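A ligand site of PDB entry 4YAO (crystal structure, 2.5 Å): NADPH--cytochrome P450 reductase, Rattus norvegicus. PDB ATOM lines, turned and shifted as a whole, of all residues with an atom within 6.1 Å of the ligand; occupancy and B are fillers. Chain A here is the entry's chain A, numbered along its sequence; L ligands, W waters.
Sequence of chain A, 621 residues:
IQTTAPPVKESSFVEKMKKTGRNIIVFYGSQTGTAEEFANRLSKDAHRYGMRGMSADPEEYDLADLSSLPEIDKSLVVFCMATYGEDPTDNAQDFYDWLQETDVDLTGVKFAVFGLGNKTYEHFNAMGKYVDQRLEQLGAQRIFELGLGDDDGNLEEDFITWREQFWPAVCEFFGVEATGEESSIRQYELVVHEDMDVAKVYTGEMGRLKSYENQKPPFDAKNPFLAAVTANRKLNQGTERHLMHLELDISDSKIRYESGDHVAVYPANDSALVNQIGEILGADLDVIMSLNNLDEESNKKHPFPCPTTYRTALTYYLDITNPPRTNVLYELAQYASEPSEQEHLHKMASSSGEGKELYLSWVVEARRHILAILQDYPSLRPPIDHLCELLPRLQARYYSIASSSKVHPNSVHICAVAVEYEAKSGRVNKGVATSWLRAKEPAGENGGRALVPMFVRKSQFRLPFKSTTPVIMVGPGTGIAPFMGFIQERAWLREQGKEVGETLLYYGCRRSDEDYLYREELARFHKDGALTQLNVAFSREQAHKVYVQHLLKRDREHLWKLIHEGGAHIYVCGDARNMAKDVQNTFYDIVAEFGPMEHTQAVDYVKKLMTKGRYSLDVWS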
ATOM      1  N   ARG A 241      38.873 -13.652 -25.801  1.00  0.00           N
ATOM      2  CA  ARG A 241      38.332 -13.219 -27.082  1.00  0.00           C
ATOM      3  C   ARG A 241      38.713 -11.774 -27.369  1.00  0.00           C
ATOM      4  O   ARG A 241      39.143 -11.039 -26.485  1.00  0.00           O
ATOM      5  CB  ARG A 241      36.817 -13.356 -27.081  1.00  0.00           C
ATOM      6  CG  ARG A 241      36.280 -14.769 -27.023  1.00  0.00           C
ATOM      7  CD  ARG A 241      34.777 -14.714 -26.757  1.00  0.00           C
ATOM      8  NE  ARG A 241      34.482 -14.037 -25.494  1.00  0.00           N
ATOM      9  CZ  ARG A 241      33.277 -13.561 -25.166  1.00  0.00           C
ATOM     10  NH1 ARG A 241      32.249 -13.694 -26.007  1.00  0.00           N
ATOM     11  NH2 ARG A 241      33.104 -12.949 -24.007  1.00  0.00           N
ATOM     12  N   PRO A 476      21.885 -10.282 -28.493  1.00  0.00           N
ATOM     13  CA  PRO A 476      23.026 -10.573 -27.623  1.00  0.00           C
ATOM     14  C   PRO A 476      24.375 -10.681 -28.375  1.00  0.00           C
ATOM     15  O   PRO A 476      24.408 -10.956 -29.589  1.00  0.00           O
ATOM     16  CB  PRO A 476      22.617 -11.884 -26.981  1.00  0.00           C
ATOM     17  CG  PRO A 476      21.874 -12.594 -28.165  1.00  0.00           C
ATOM     18  CD  PRO A 476      21.018 -11.474 -28.671  1.00  0.00           C
ATOM     19  N   GLY A 477      25.476 -10.461 -27.649  1.00  0.00           N
ATOM     20  CA  GLY A 477      26.808 -10.531 -28.240  1.00  0.00           C
ATOM     21  C   GLY A 477      26.983  -9.519 -29.353  1.00  0.00           C
ATOM     22  O   GLY A 477      26.592  -8.368 -29.180  1.00  0.00           O
ATOM     23  N   THR A 478      27.573  -9.920 -30.475  1.00  0.00           N
ATOM     24  CA  THR A 478      27.729  -8.984 -31.597  1.00  0.00           C
ATOM     25  C   THR A 478      26.398  -8.507 -32.185  1.00  0.00           C
ATOM     26  O   THR A 478      26.363  -7.494 -32.890  1.00  0.00           O
ATOM     27  CB  THR A 478      28.571  -9.563 -32.768  1.00  0.00           C
ATOM     28  OG1 THR A 478      28.252 -10.936 -32.972  1.00  0.00           O
ATOM     29  CG2 THR A 478      30.056  -9.393 -32.504  1.00  0.00           C
ATOM     30  N   GLY A 508      22.824  -8.960 -24.226  1.00  0.00           N
ATOM     31  CA  GLY A 508      23.393  -9.996 -23.387  1.00  0.00           C
ATOM     32  C   GLY A 508      24.849 -10.300 -23.653  1.00  0.00           C
ATOM     33  O   GLY A 508      25.313 -10.262 -24.791  1.00  0.00           O
ATOM     34  N   CYS A 509      25.566 -10.636 -22.580  1.00  0.00           N
ATOM     35  CA  CYS A 509      26.977 -10.974 -22.662  1.00  0.00           C
ATOM     36  C   CYS A 509      27.284 -11.924 -21.506  1.00  0.00           C
ATOM     37  O   CYS A 509      26.388 -12.232 -20.710  1.00  0.00           O
ATOM     38  CB  CYS A 509      27.819  -9.696 -22.535  1.00  0.00           C
ATOM     39  SG  CYS A 509      27.555  -8.888 -20.970  1.00  0.00           S
ATOM     40  N   ARG A 510      28.526 -12.400 -21.392  1.00  0.00           N
ATOM     41  CA  ARG A 510      28.904 -13.284 -20.283  1.00  0.00           C
ATOM     42  C   ARG A 510      28.802 -12.601 -18.920  1.00  0.00           C
ATOM     43  O   ARG A 510      27.946 -12.957 -18.090  1.00  0.00           O
ATOM     44  CB  ARG A 510      30.325 -13.807 -20.492  1.00  0.00           C
ATOM     45  CG  ARG A 510      30.424 -14.651 -21.750  1.00  0.00           C
ATOM     46  CD  ARG A 510      31.810 -15.168 -22.051  1.00  0.00           C
ATOM     47  NE  ARG A 510      31.836 -15.787 -23.376  1.00  0.00           N
ATOM     48  CZ  ARG A 510      32.827 -16.531 -23.846  1.00  0.00           C
ATOM     49  NH1 ARG A 510      33.899 -16.775 -23.094  1.00  0.00           N
ATOM     50  NH2 ARG A 510      32.742 -17.053 -25.065  1.00  0.00           N
ATOM     51  N   ASP A 515      32.675  -8.353 -20.898  1.00  0.00           N
ATOM     52  CA  ASP A 515      32.356  -8.171 -22.303  1.00  0.00           C
ATOM     53  C   ASP A 515      31.012  -7.505 -22.612  1.00  0.00           C
ATOM     54  O   ASP A 515      30.343  -7.852 -23.587  1.00  0.00           O
ATOM     55  CB  ASP A 515      32.476  -9.517 -23.038  1.00  0.00           C
ATOM     56  CG  ASP A 515      31.459 -10.533 -22.582  1.00  0.00           C
ATOM     57  OD1 ASP A 515      30.881 -10.369 -21.485  1.00  0.00           O
ATOM     58  OD2 ASP A 515      31.242 -11.507 -23.338  1.00  0.00           O
ATOM     59  N   ALA A 537      21.288  -9.352 -20.042  1.00  0.00           N
ATOM     60  CA  ALA A 537      21.259 -10.685 -19.463  1.00  0.00           C
ATOM     61  C   ALA A 537      22.718 -11.104 -19.302  1.00  0.00           C
ATOM     62  O   ALA A 537      23.466 -11.142 -20.284  1.00  0.00           O
ATOM     63  CB  ALA A 537      20.518 -11.657 -20.380  1.00  0.00           C
ATOM     64  N   PHE A 538      23.126 -11.343 -18.070  1.00  0.00           N
ATOM     65  CA  PHE A 538      24.495 -11.771 -17.814  1.00  0.00           C
ATOM     66  C   PHE A 538      24.479 -13.287 -17.686  1.00  0.00           C
ATOM     67  O   PHE A 538      24.133 -13.852 -16.640  1.00  0.00           O
ATOM     68  CB  PHE A 538      25.029 -11.079 -16.554  1.00  0.00           C
ATOM     69  CG  PHE A 538      25.092  -9.582 -16.689  1.00  0.00           C
ATOM     70  CD1 PHE A 538      25.808  -8.986 -17.727  1.00  0.00           C
ATOM     71  CD2 PHE A 538      24.385  -8.756 -15.824  1.00  0.00           C
ATOM     72  CE1 PHE A 538      25.806  -7.612 -17.898  1.00  0.00           C
ATOM     73  CE2 PHE A 538      24.383  -7.382 -15.994  1.00  0.00           C
ATOM     74  CZ  PHE A 538      25.094  -6.809 -17.032  1.00  0.00           C
ATOM     75  N   SER A 539      24.833 -13.942 -18.787  1.00  0.00           N
ATOM     76  CA  SER A 539      24.816 -15.382 -18.882  1.00  0.00           C
ATOM     77  C   SER A 539      25.557 -16.174 -17.822  1.00  0.00           C
ATOM     78  O   SER A 539      25.008 -17.148 -17.289  1.00  0.00           O
ATOM     79  CB  SER A 539      25.303 -15.810 -20.275  1.00  0.00           C
ATOM     80  OG  SER A 539      26.603 -15.311 -20.534  1.00  0.00           O
ATOM     81  N   ARG A 540      26.792 -15.772 -17.512  1.00  0.00           N
ATOM     82  CA  ARG A 540      27.628 -16.499 -16.560  1.00  0.00           C
ATOM     83  C   ARG A 540      27.733 -15.958 -15.145  1.00  0.00           C
ATOM     84  O   ARG A 540      28.445 -16.527 -14.317  1.00  0.00           O
ATOM     85  CB  ARG A 540      29.023 -16.636 -17.138  1.00  0.00           C
ATOM     86  CG  ARG A 540      28.998 -17.136 -18.541  1.00  0.00           C
ATOM     87  CD  ARG A 540      30.355 -17.549 -19.029  1.00  0.00           C
ATOM     88  NE  ARG A 540      30.265 -17.934 -20.429  1.00  0.00           N
ATOM     89  CZ  ARG A 540      31.248 -18.511 -21.102  1.00  0.00           C
ATOM     90  NH1 ARG A 540      32.393 -18.785 -20.507  1.00  0.00           N
ATOM     91  NH2 ARG A 540      31.076 -18.810 -22.393  1.00  0.00           N
ATOM     92  N   LYS A 545      22.113 -20.205 -16.755  1.00  0.00           N
ATOM     93  CA  LYS A 545      22.442 -19.304 -17.850  1.00  0.00           C
ATOM     94  C   LYS A 545      21.226 -18.371 -17.917  1.00  0.00           C
ATOM     95  O   LYS A 545      20.105 -18.851 -17.926  1.00  0.00           O
ATOM     96  CB  LYS A 545      22.517 -20.059 -19.190  1.00  0.00           C
ATOM     97  CG  LYS A 545      23.678 -21.023 -19.373  1.00  0.00           C
ATOM     98  CD  LYS A 545      24.934 -20.308 -19.804  1.00  0.00           C
ATOM     99  CE  LYS A 545      26.010 -21.275 -20.224  1.00  0.00           C
ATOM    100  NZ  LYS A 545      27.301 -20.539 -20.381  1.00  0.00           N
ATOM    101  N   VAL A 546      21.439 -17.064 -17.955  1.00  0.00           N
ATOM    102  CA  VAL A 546      20.305 -16.153 -18.098  1.00  0.00           C
ATOM    103  C   VAL A 546      20.493 -15.517 -19.469  1.00  0.00           C
ATOM    104  O   VAL A 546      21.470 -14.819 -19.698  1.00  0.00           O
ATOM    105  CB  VAL A 546      20.274 -15.092 -16.967  1.00  0.00           C
ATOM    106  CG1 VAL A 546      19.294 -13.995 -17.303  1.00  0.00           C
ATOM    107  CG2 VAL A 546      19.869 -15.732 -15.667  1.00  0.00           C
ATOM    108  N   TYR A 547      19.581 -15.809 -20.382  1.00  0.00           N
ATOM    109  CA  TYR A 547      19.683 -15.275 -21.743  1.00  0.00           C
ATOM    110  C   TYR A 547      18.621 -14.225 -22.027  1.00  0.00           C
ATOM    111  O   TYR A 547      17.706 -14.035 -21.225  1.00  0.00           O
ATOM    112  CB  TYR A 547      19.550 -16.411 -22.754  1.00  0.00           C
ATOM    113  CG  TYR A 547      20.656 -17.445 -22.671  1.00  0.00           C
ATOM    114  CD1 TYR A 547      21.995 -17.061 -22.582  1.00  0.00           C
ATOM    115  CD2 TYR A 547      20.380 -18.814 -22.788  1.00  0.00           C
ATOM    116  CE1 TYR A 547      23.015 -18.003 -22.605  1.00  0.00           C
ATOM    117  CE2 TYR A 547      21.401 -19.773 -22.806  1.00  0.00           C
ATOM    118  CZ  TYR A 547      22.709 -19.361 -22.725  1.00  0.00           C
ATOM    119  OH  TYR A 547      23.725 -20.277 -22.740  1.00  0.00           O
ATOM    120  N   VAL A 548      18.739 -13.527 -23.154  1.00  0.00           N
ATOM    121  CA  VAL A 548      17.763 -12.493 -23.479  1.00  0.00           C
ATOM    122  C   VAL A 548      16.314 -12.964 -23.450  1.00  0.00           C
ATOM    123  O   VAL A 548      15.453 -12.247 -22.960  1.00  0.00           O
ATOM    124  CB  VAL A 548      18.048 -11.827 -24.839  1.00  0.00           C
ATOM    125  CG1 VAL A 548      19.145 -10.777 -24.692  1.00  0.00           C
ATOM    126  CG2 VAL A 548      18.464 -12.875 -25.847  1.00  0.00           C
ATOM    127  N   GLN A 549      16.036 -14.185 -23.927  1.00  0.00           N
ATOM    128  CA  GLN A 549      14.668 -14.697 -23.937  1.00  0.00           C
ATOM    129  C   GLN A 549      14.081 -14.879 -22.552  1.00  0.00           C
ATOM    130  O   GLN A 549      12.857 -14.898 -22.390  1.00  0.00           O
ATOM    131  CB  GLN A 549      14.558 -16.017 -24.704  1.00  0.00           C
ATOM    132  CG  GLN A 549      15.392 -17.151 -24.164  1.00  0.00           C
ATOM    133  CD  GLN A 549      16.763 -17.185 -24.777  1.00  0.00           C
ATOM    134  OE1 GLN A 549      17.271 -16.169 -25.229  1.00  0.00           O
ATOM    135  NE2 GLN A 549      17.356 -18.370 -24.808  1.00  0.00           N
ATOM    136  N   ASP A 575      23.474 -14.523 -33.393  1.00  0.00           N
ATOM    137  CA  ASP A 575      23.435 -15.953 -33.684  1.00  0.00           C
ATOM    138  C   ASP A 575      22.099 -16.498 -34.250  1.00  0.00           C
ATOM    139  O   ASP A 575      21.063 -16.381 -33.631  1.00  0.00           O
ATOM    140  CB  ASP A 575      23.780 -16.736 -32.407  1.00  0.00           C
ATOM    141  CG  ASP A 575      23.584 -18.230 -32.582  1.00  0.00           C
ATOM    142  OD1 ASP A 575      24.294 -18.817 -33.417  1.00  0.00           O
ATOM    143  OD2 ASP A 575      22.713 -18.804 -31.885  1.00  0.00           O
ATOM    144  N   ASN A 578      20.935 -20.838 -32.724  1.00  0.00           N
ATOM    145  CA  ASN A 578      20.037 -21.145 -31.614  1.00  0.00           C
ATOM    146  C   ASN A 578      19.328 -19.937 -31.039  1.00  0.00           C
ATOM    147  O   ASN A 578      18.100 -19.925 -30.932  1.00  0.00           O
ATOM    148  CB  ASN A 578      20.816 -21.821 -30.495  1.00  0.00           C
ATOM    149  CG  ASN A 578      21.587 -23.016 -30.976  1.00  0.00           C
ATOM    150  OD1 ASN A 578      22.337 -22.934 -31.959  1.00  0.00           O
ATOM    151  ND2 ASN A 578      21.438 -24.145 -30.277  1.00  0.00           N
ATOM    152  N   MET A 579      20.098 -18.919 -30.673  1.00  0.00           N
ATOM    153  CA  MET A 579      19.544 -17.722 -30.066  1.00  0.00           C
ATOM    154  C   MET A 579      18.264 -17.206 -30.726  1.00  0.00           C
ATOM    155  O   MET A 579      17.287 -16.926 -30.036  1.00  0.00           O
ATOM    156  CB  MET A 579      20.594 -16.611 -30.049  1.00  0.00           C
ATOM    157  CG  MET A 579      20.110 -15.284 -29.456  1.00  0.00           C
ATOM    158  SD  MET A 579      19.113 -14.263 -30.559  1.00  0.00           S
ATOM    159  CE  MET A 579      17.817 -14.007 -29.571  1.00  0.00           C
ATOM    160  N   ALA A 580      18.286 -17.071 -32.039  1.00  0.00           N
ATOM    161  CA  ALA A 580      17.130 -16.569 -32.773  1.00  0.00           C
ATOM    162  C   ALA A 580      15.935 -17.526 -32.694  1.00  0.00           C
ATOM    163  O   ALA A 580      14.796 -17.086 -32.602  1.00  0.00           O
ATOM    164  CB  ALA A 580      17.504 -16.286 -34.226  1.00  0.00           C
ATOM    165  N   ASP A 582      15.362 -19.712 -30.229  1.00  0.00           N
ATOM    166  CA  ASP A 582      14.904 -19.650 -28.849  1.00  0.00           C
ATOM    167  C   ASP A 582      14.044 -18.432 -28.596  1.00  0.00           C
ATOM    168  O   ASP A 582      13.033 -18.537 -27.897  1.00  0.00           O
ATOM    169  CB  ASP A 582      16.070 -19.656 -27.885  1.00  0.00           C
ATOM    170  CG  ASP A 582      16.741 -21.014 -27.774  1.00  0.00           C
ATOM    171  OD1 ASP A 582      16.087 -22.045 -28.075  1.00  0.00           O
ATOM    172  OD2 ASP A 582      17.918 -21.066 -27.365  1.00  0.00           O
ATOM    173  N   VAL A 583      14.418 -17.289 -29.152  1.00  0.00           N
ATOM    174  CA  VAL A 583      13.622 -16.083 -28.944  1.00  0.00           C
ATOM    175  C   VAL A 583      12.293 -16.139 -29.684  1.00  0.00           C
ATOM    176  O   VAL A 583      11.276 -15.669 -29.197  1.00  0.00           O
ATOM    177  CB  VAL A 583      14.404 -14.797 -29.348  1.00  0.00           C
ATOM    178  CG1 VAL A 583      13.455 -13.645 -29.625  1.00  0.00           C
ATOM    179  CG2 VAL A 583      15.297 -14.405 -28.209  1.00  0.00           C
HETATM  180  P1  LIG L   1      26.930 -18.234 -22.887  1.00  0.00           P
HETATM  181  O1  LIG L   1      27.169 -18.275 -21.429  1.00  0.00           O
HETATM  182  O2  LIG L   1      26.066 -19.324 -23.397  1.00  0.00           O
HETATM  183  O3  LIG L   1      28.162 -18.027 -23.685  1.00  0.00           O
HETATM  184  C1  LIG L   1      26.737 -13.434 -26.291  1.00  0.00           C
HETATM  185  O4  LIG L   1      27.492 -14.493 -26.880  1.00  0.00           O
HETATM  186  C2  LIG L   1      25.755 -13.986 -25.265  1.00  0.00           C
HETATM  187  O5  LIG L   1      24.873 -14.961 -25.868  1.00  0.00           O
HETATM  188  C3  LIG L   1      26.475 -14.725 -24.148  1.00  0.00           C
HETATM  189  O6  LIG L   1      25.961 -14.261 -22.889  1.00  0.00           O
HETATM  190  C4  LIG L   1      26.053 -16.172 -24.347  1.00  0.00           C
HETATM  191  O7  LIG L   1      26.075 -16.889 -23.098  1.00  0.00           O
HETATM  192  C5  LIG L   1      24.639 -15.915 -24.835  1.00  0.00           C
HETATM  193  N1  LIG L   1      23.986 -17.120 -25.403  1.00  0.00           N
HETATM  194  C6  LIG L   1      24.558 -18.272 -25.730  1.00  0.00           C
HETATM  195  N2  LIG L   1      23.620 -19.055 -26.257  1.00  0.00           N
HETATM  196  C7  LIG L   1      22.472 -18.388 -26.250  1.00  0.00           C
HETATM  197  C8  LIG L   1      21.238 -18.772 -26.543  1.00  0.00           C
HETATM  198  N3  LIG L   1      21.076 -20.044 -26.882  1.00  0.00           N
HETATM  199  N4  LIG L   1      20.186 -17.947 -26.405  1.00  0.00           N
HETATM  200  C9  LIG L   1      20.410 -16.644 -25.955  1.00  0.00           C
HETATM  201  N5  LIG L   1      21.721 -16.275 -25.639  1.00  0.00           N
HETATM  202  C10 LIG L   1      22.707 -17.174 -25.774  1.00  0.00           C
HETATM  203  O   HOH W   1      29.341 -11.856 -25.610  1.00  0.00           O
HETATM  204  O   HOH W   2      29.025 -21.125 -22.189  1.00  0.00           O
HETATM  205  O   HOH W   3      23.670 -13.477 -22.525  1.00  0.00           O
HETATM  206  O   HOH W   4      29.695 -16.125 -25.243  1.00  0.00           O
HETATM  207  O   HOH W   5      24.827 -21.850 -27.231  1.00  0.00           O
HETATM  208  O   HOH W   6      21.890 -22.962 -26.028  1.00  0.00           O
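The side-chain amino group (NZ) of Lys 545 lies within salt-bridge range of an oxygen (O1) of the ligand (2.5 Å).
An oxygen (O2) of the ligand sits at hydrogen-bond distance from the side-chain hydroxyl (OH) of Tyr 547 (2.6 Å).
O6 of the ligand sits at hydrogen-bond distance from OG of Ser 539 (2.7 Å).
O6 of the ligand is in hydrogen-bond range of O of Cys 509, 3.0 Å away.
A nitrogen (N4) of the ligand sits at hydrogen-bond distance from the side-chain amide nitrogen (NE2) of Gln 549, 3.3 Å away.
NE of Arg 540 lies within salt-bridge range of O1 of the ligand (3.3 Å).
N3 of the ligand is in hydrogen-bond range of OD2 of Asp 582 (3.4 Å).
The backbone NH (N) of Ser 539 lies within hydrogen-bond range of the backbone carbonyl oxygen (O) of Cys 509, 3.0 Å away.
The backbone NH of Ser 539 lies within hydrogen-bond range of the backbone carbonyl oxygen of Arg 510, at 3.3 Å.
The backbone carbonyl oxygen (O) of Ala 537 sits at hydrogen-bond distance from the backbone NH (N) of Cys 509 (3.2 Å).
The side-chain carboxylate (OD1) of Asp 515 lies close to the side-chain sulfur (SG) of Cys 509 (3.7 Å).
O of Arg 510 lies within hydrogen-bond range of N of Arg 540 (3.1 Å).
The backbone NH (N) of Gly 477 is in hydrogen-bond range of the backbone carbonyl oxygen (O) of Gly 508 (2.9 Å).
OD1 of Asp 515 is in hydrogen-bond range of N of Arg 510 (3.1 Å).
N of Met 579 lies within hydrogen-bond range of OD2 of Asp 575 (2.9 Å).
Residues that only touch the ligand: Gly 477, Arg 510, Met 579, Gly 508 and Pro 476.
Hydrophobic or aromatic side chains within 4 Å of the ligand: Pro 476, Tyr 547 and Met 579.
The nearest printed residue that does not touch the ligand is Asn 578 (4.03 Å).
Water W3 lies within hydrogen-bond range of O6 of the ligand (2.4 Å), O of Ala 537 (3.2 Å) and N of Cys 509 (3.4 Å).
Water W4 lies within hydrogen-bond range of the guanidinium group (NE) of Arg 510 (2.9 Å) and an oxygen (O3) of the ligand (2.9 Å).
Water W1 lies within hydrogen-bond range of the side-chain carboxylate (OD2) of Asp 515 (3.0 Å), an oxygen (O4) of the ligand (3.5 Å) and the guanidinium group (NH1) of Arg 241 (3.5 Å).
Water W2 lies within hydrogen-bond range of the side-chain amino group (NZ) of Lys 545 (2.6 Å), the guanidinium group (NH2) of Arg 540 (3.1 Å) and an oxygen (O1) of the ligand (3.5 Å).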
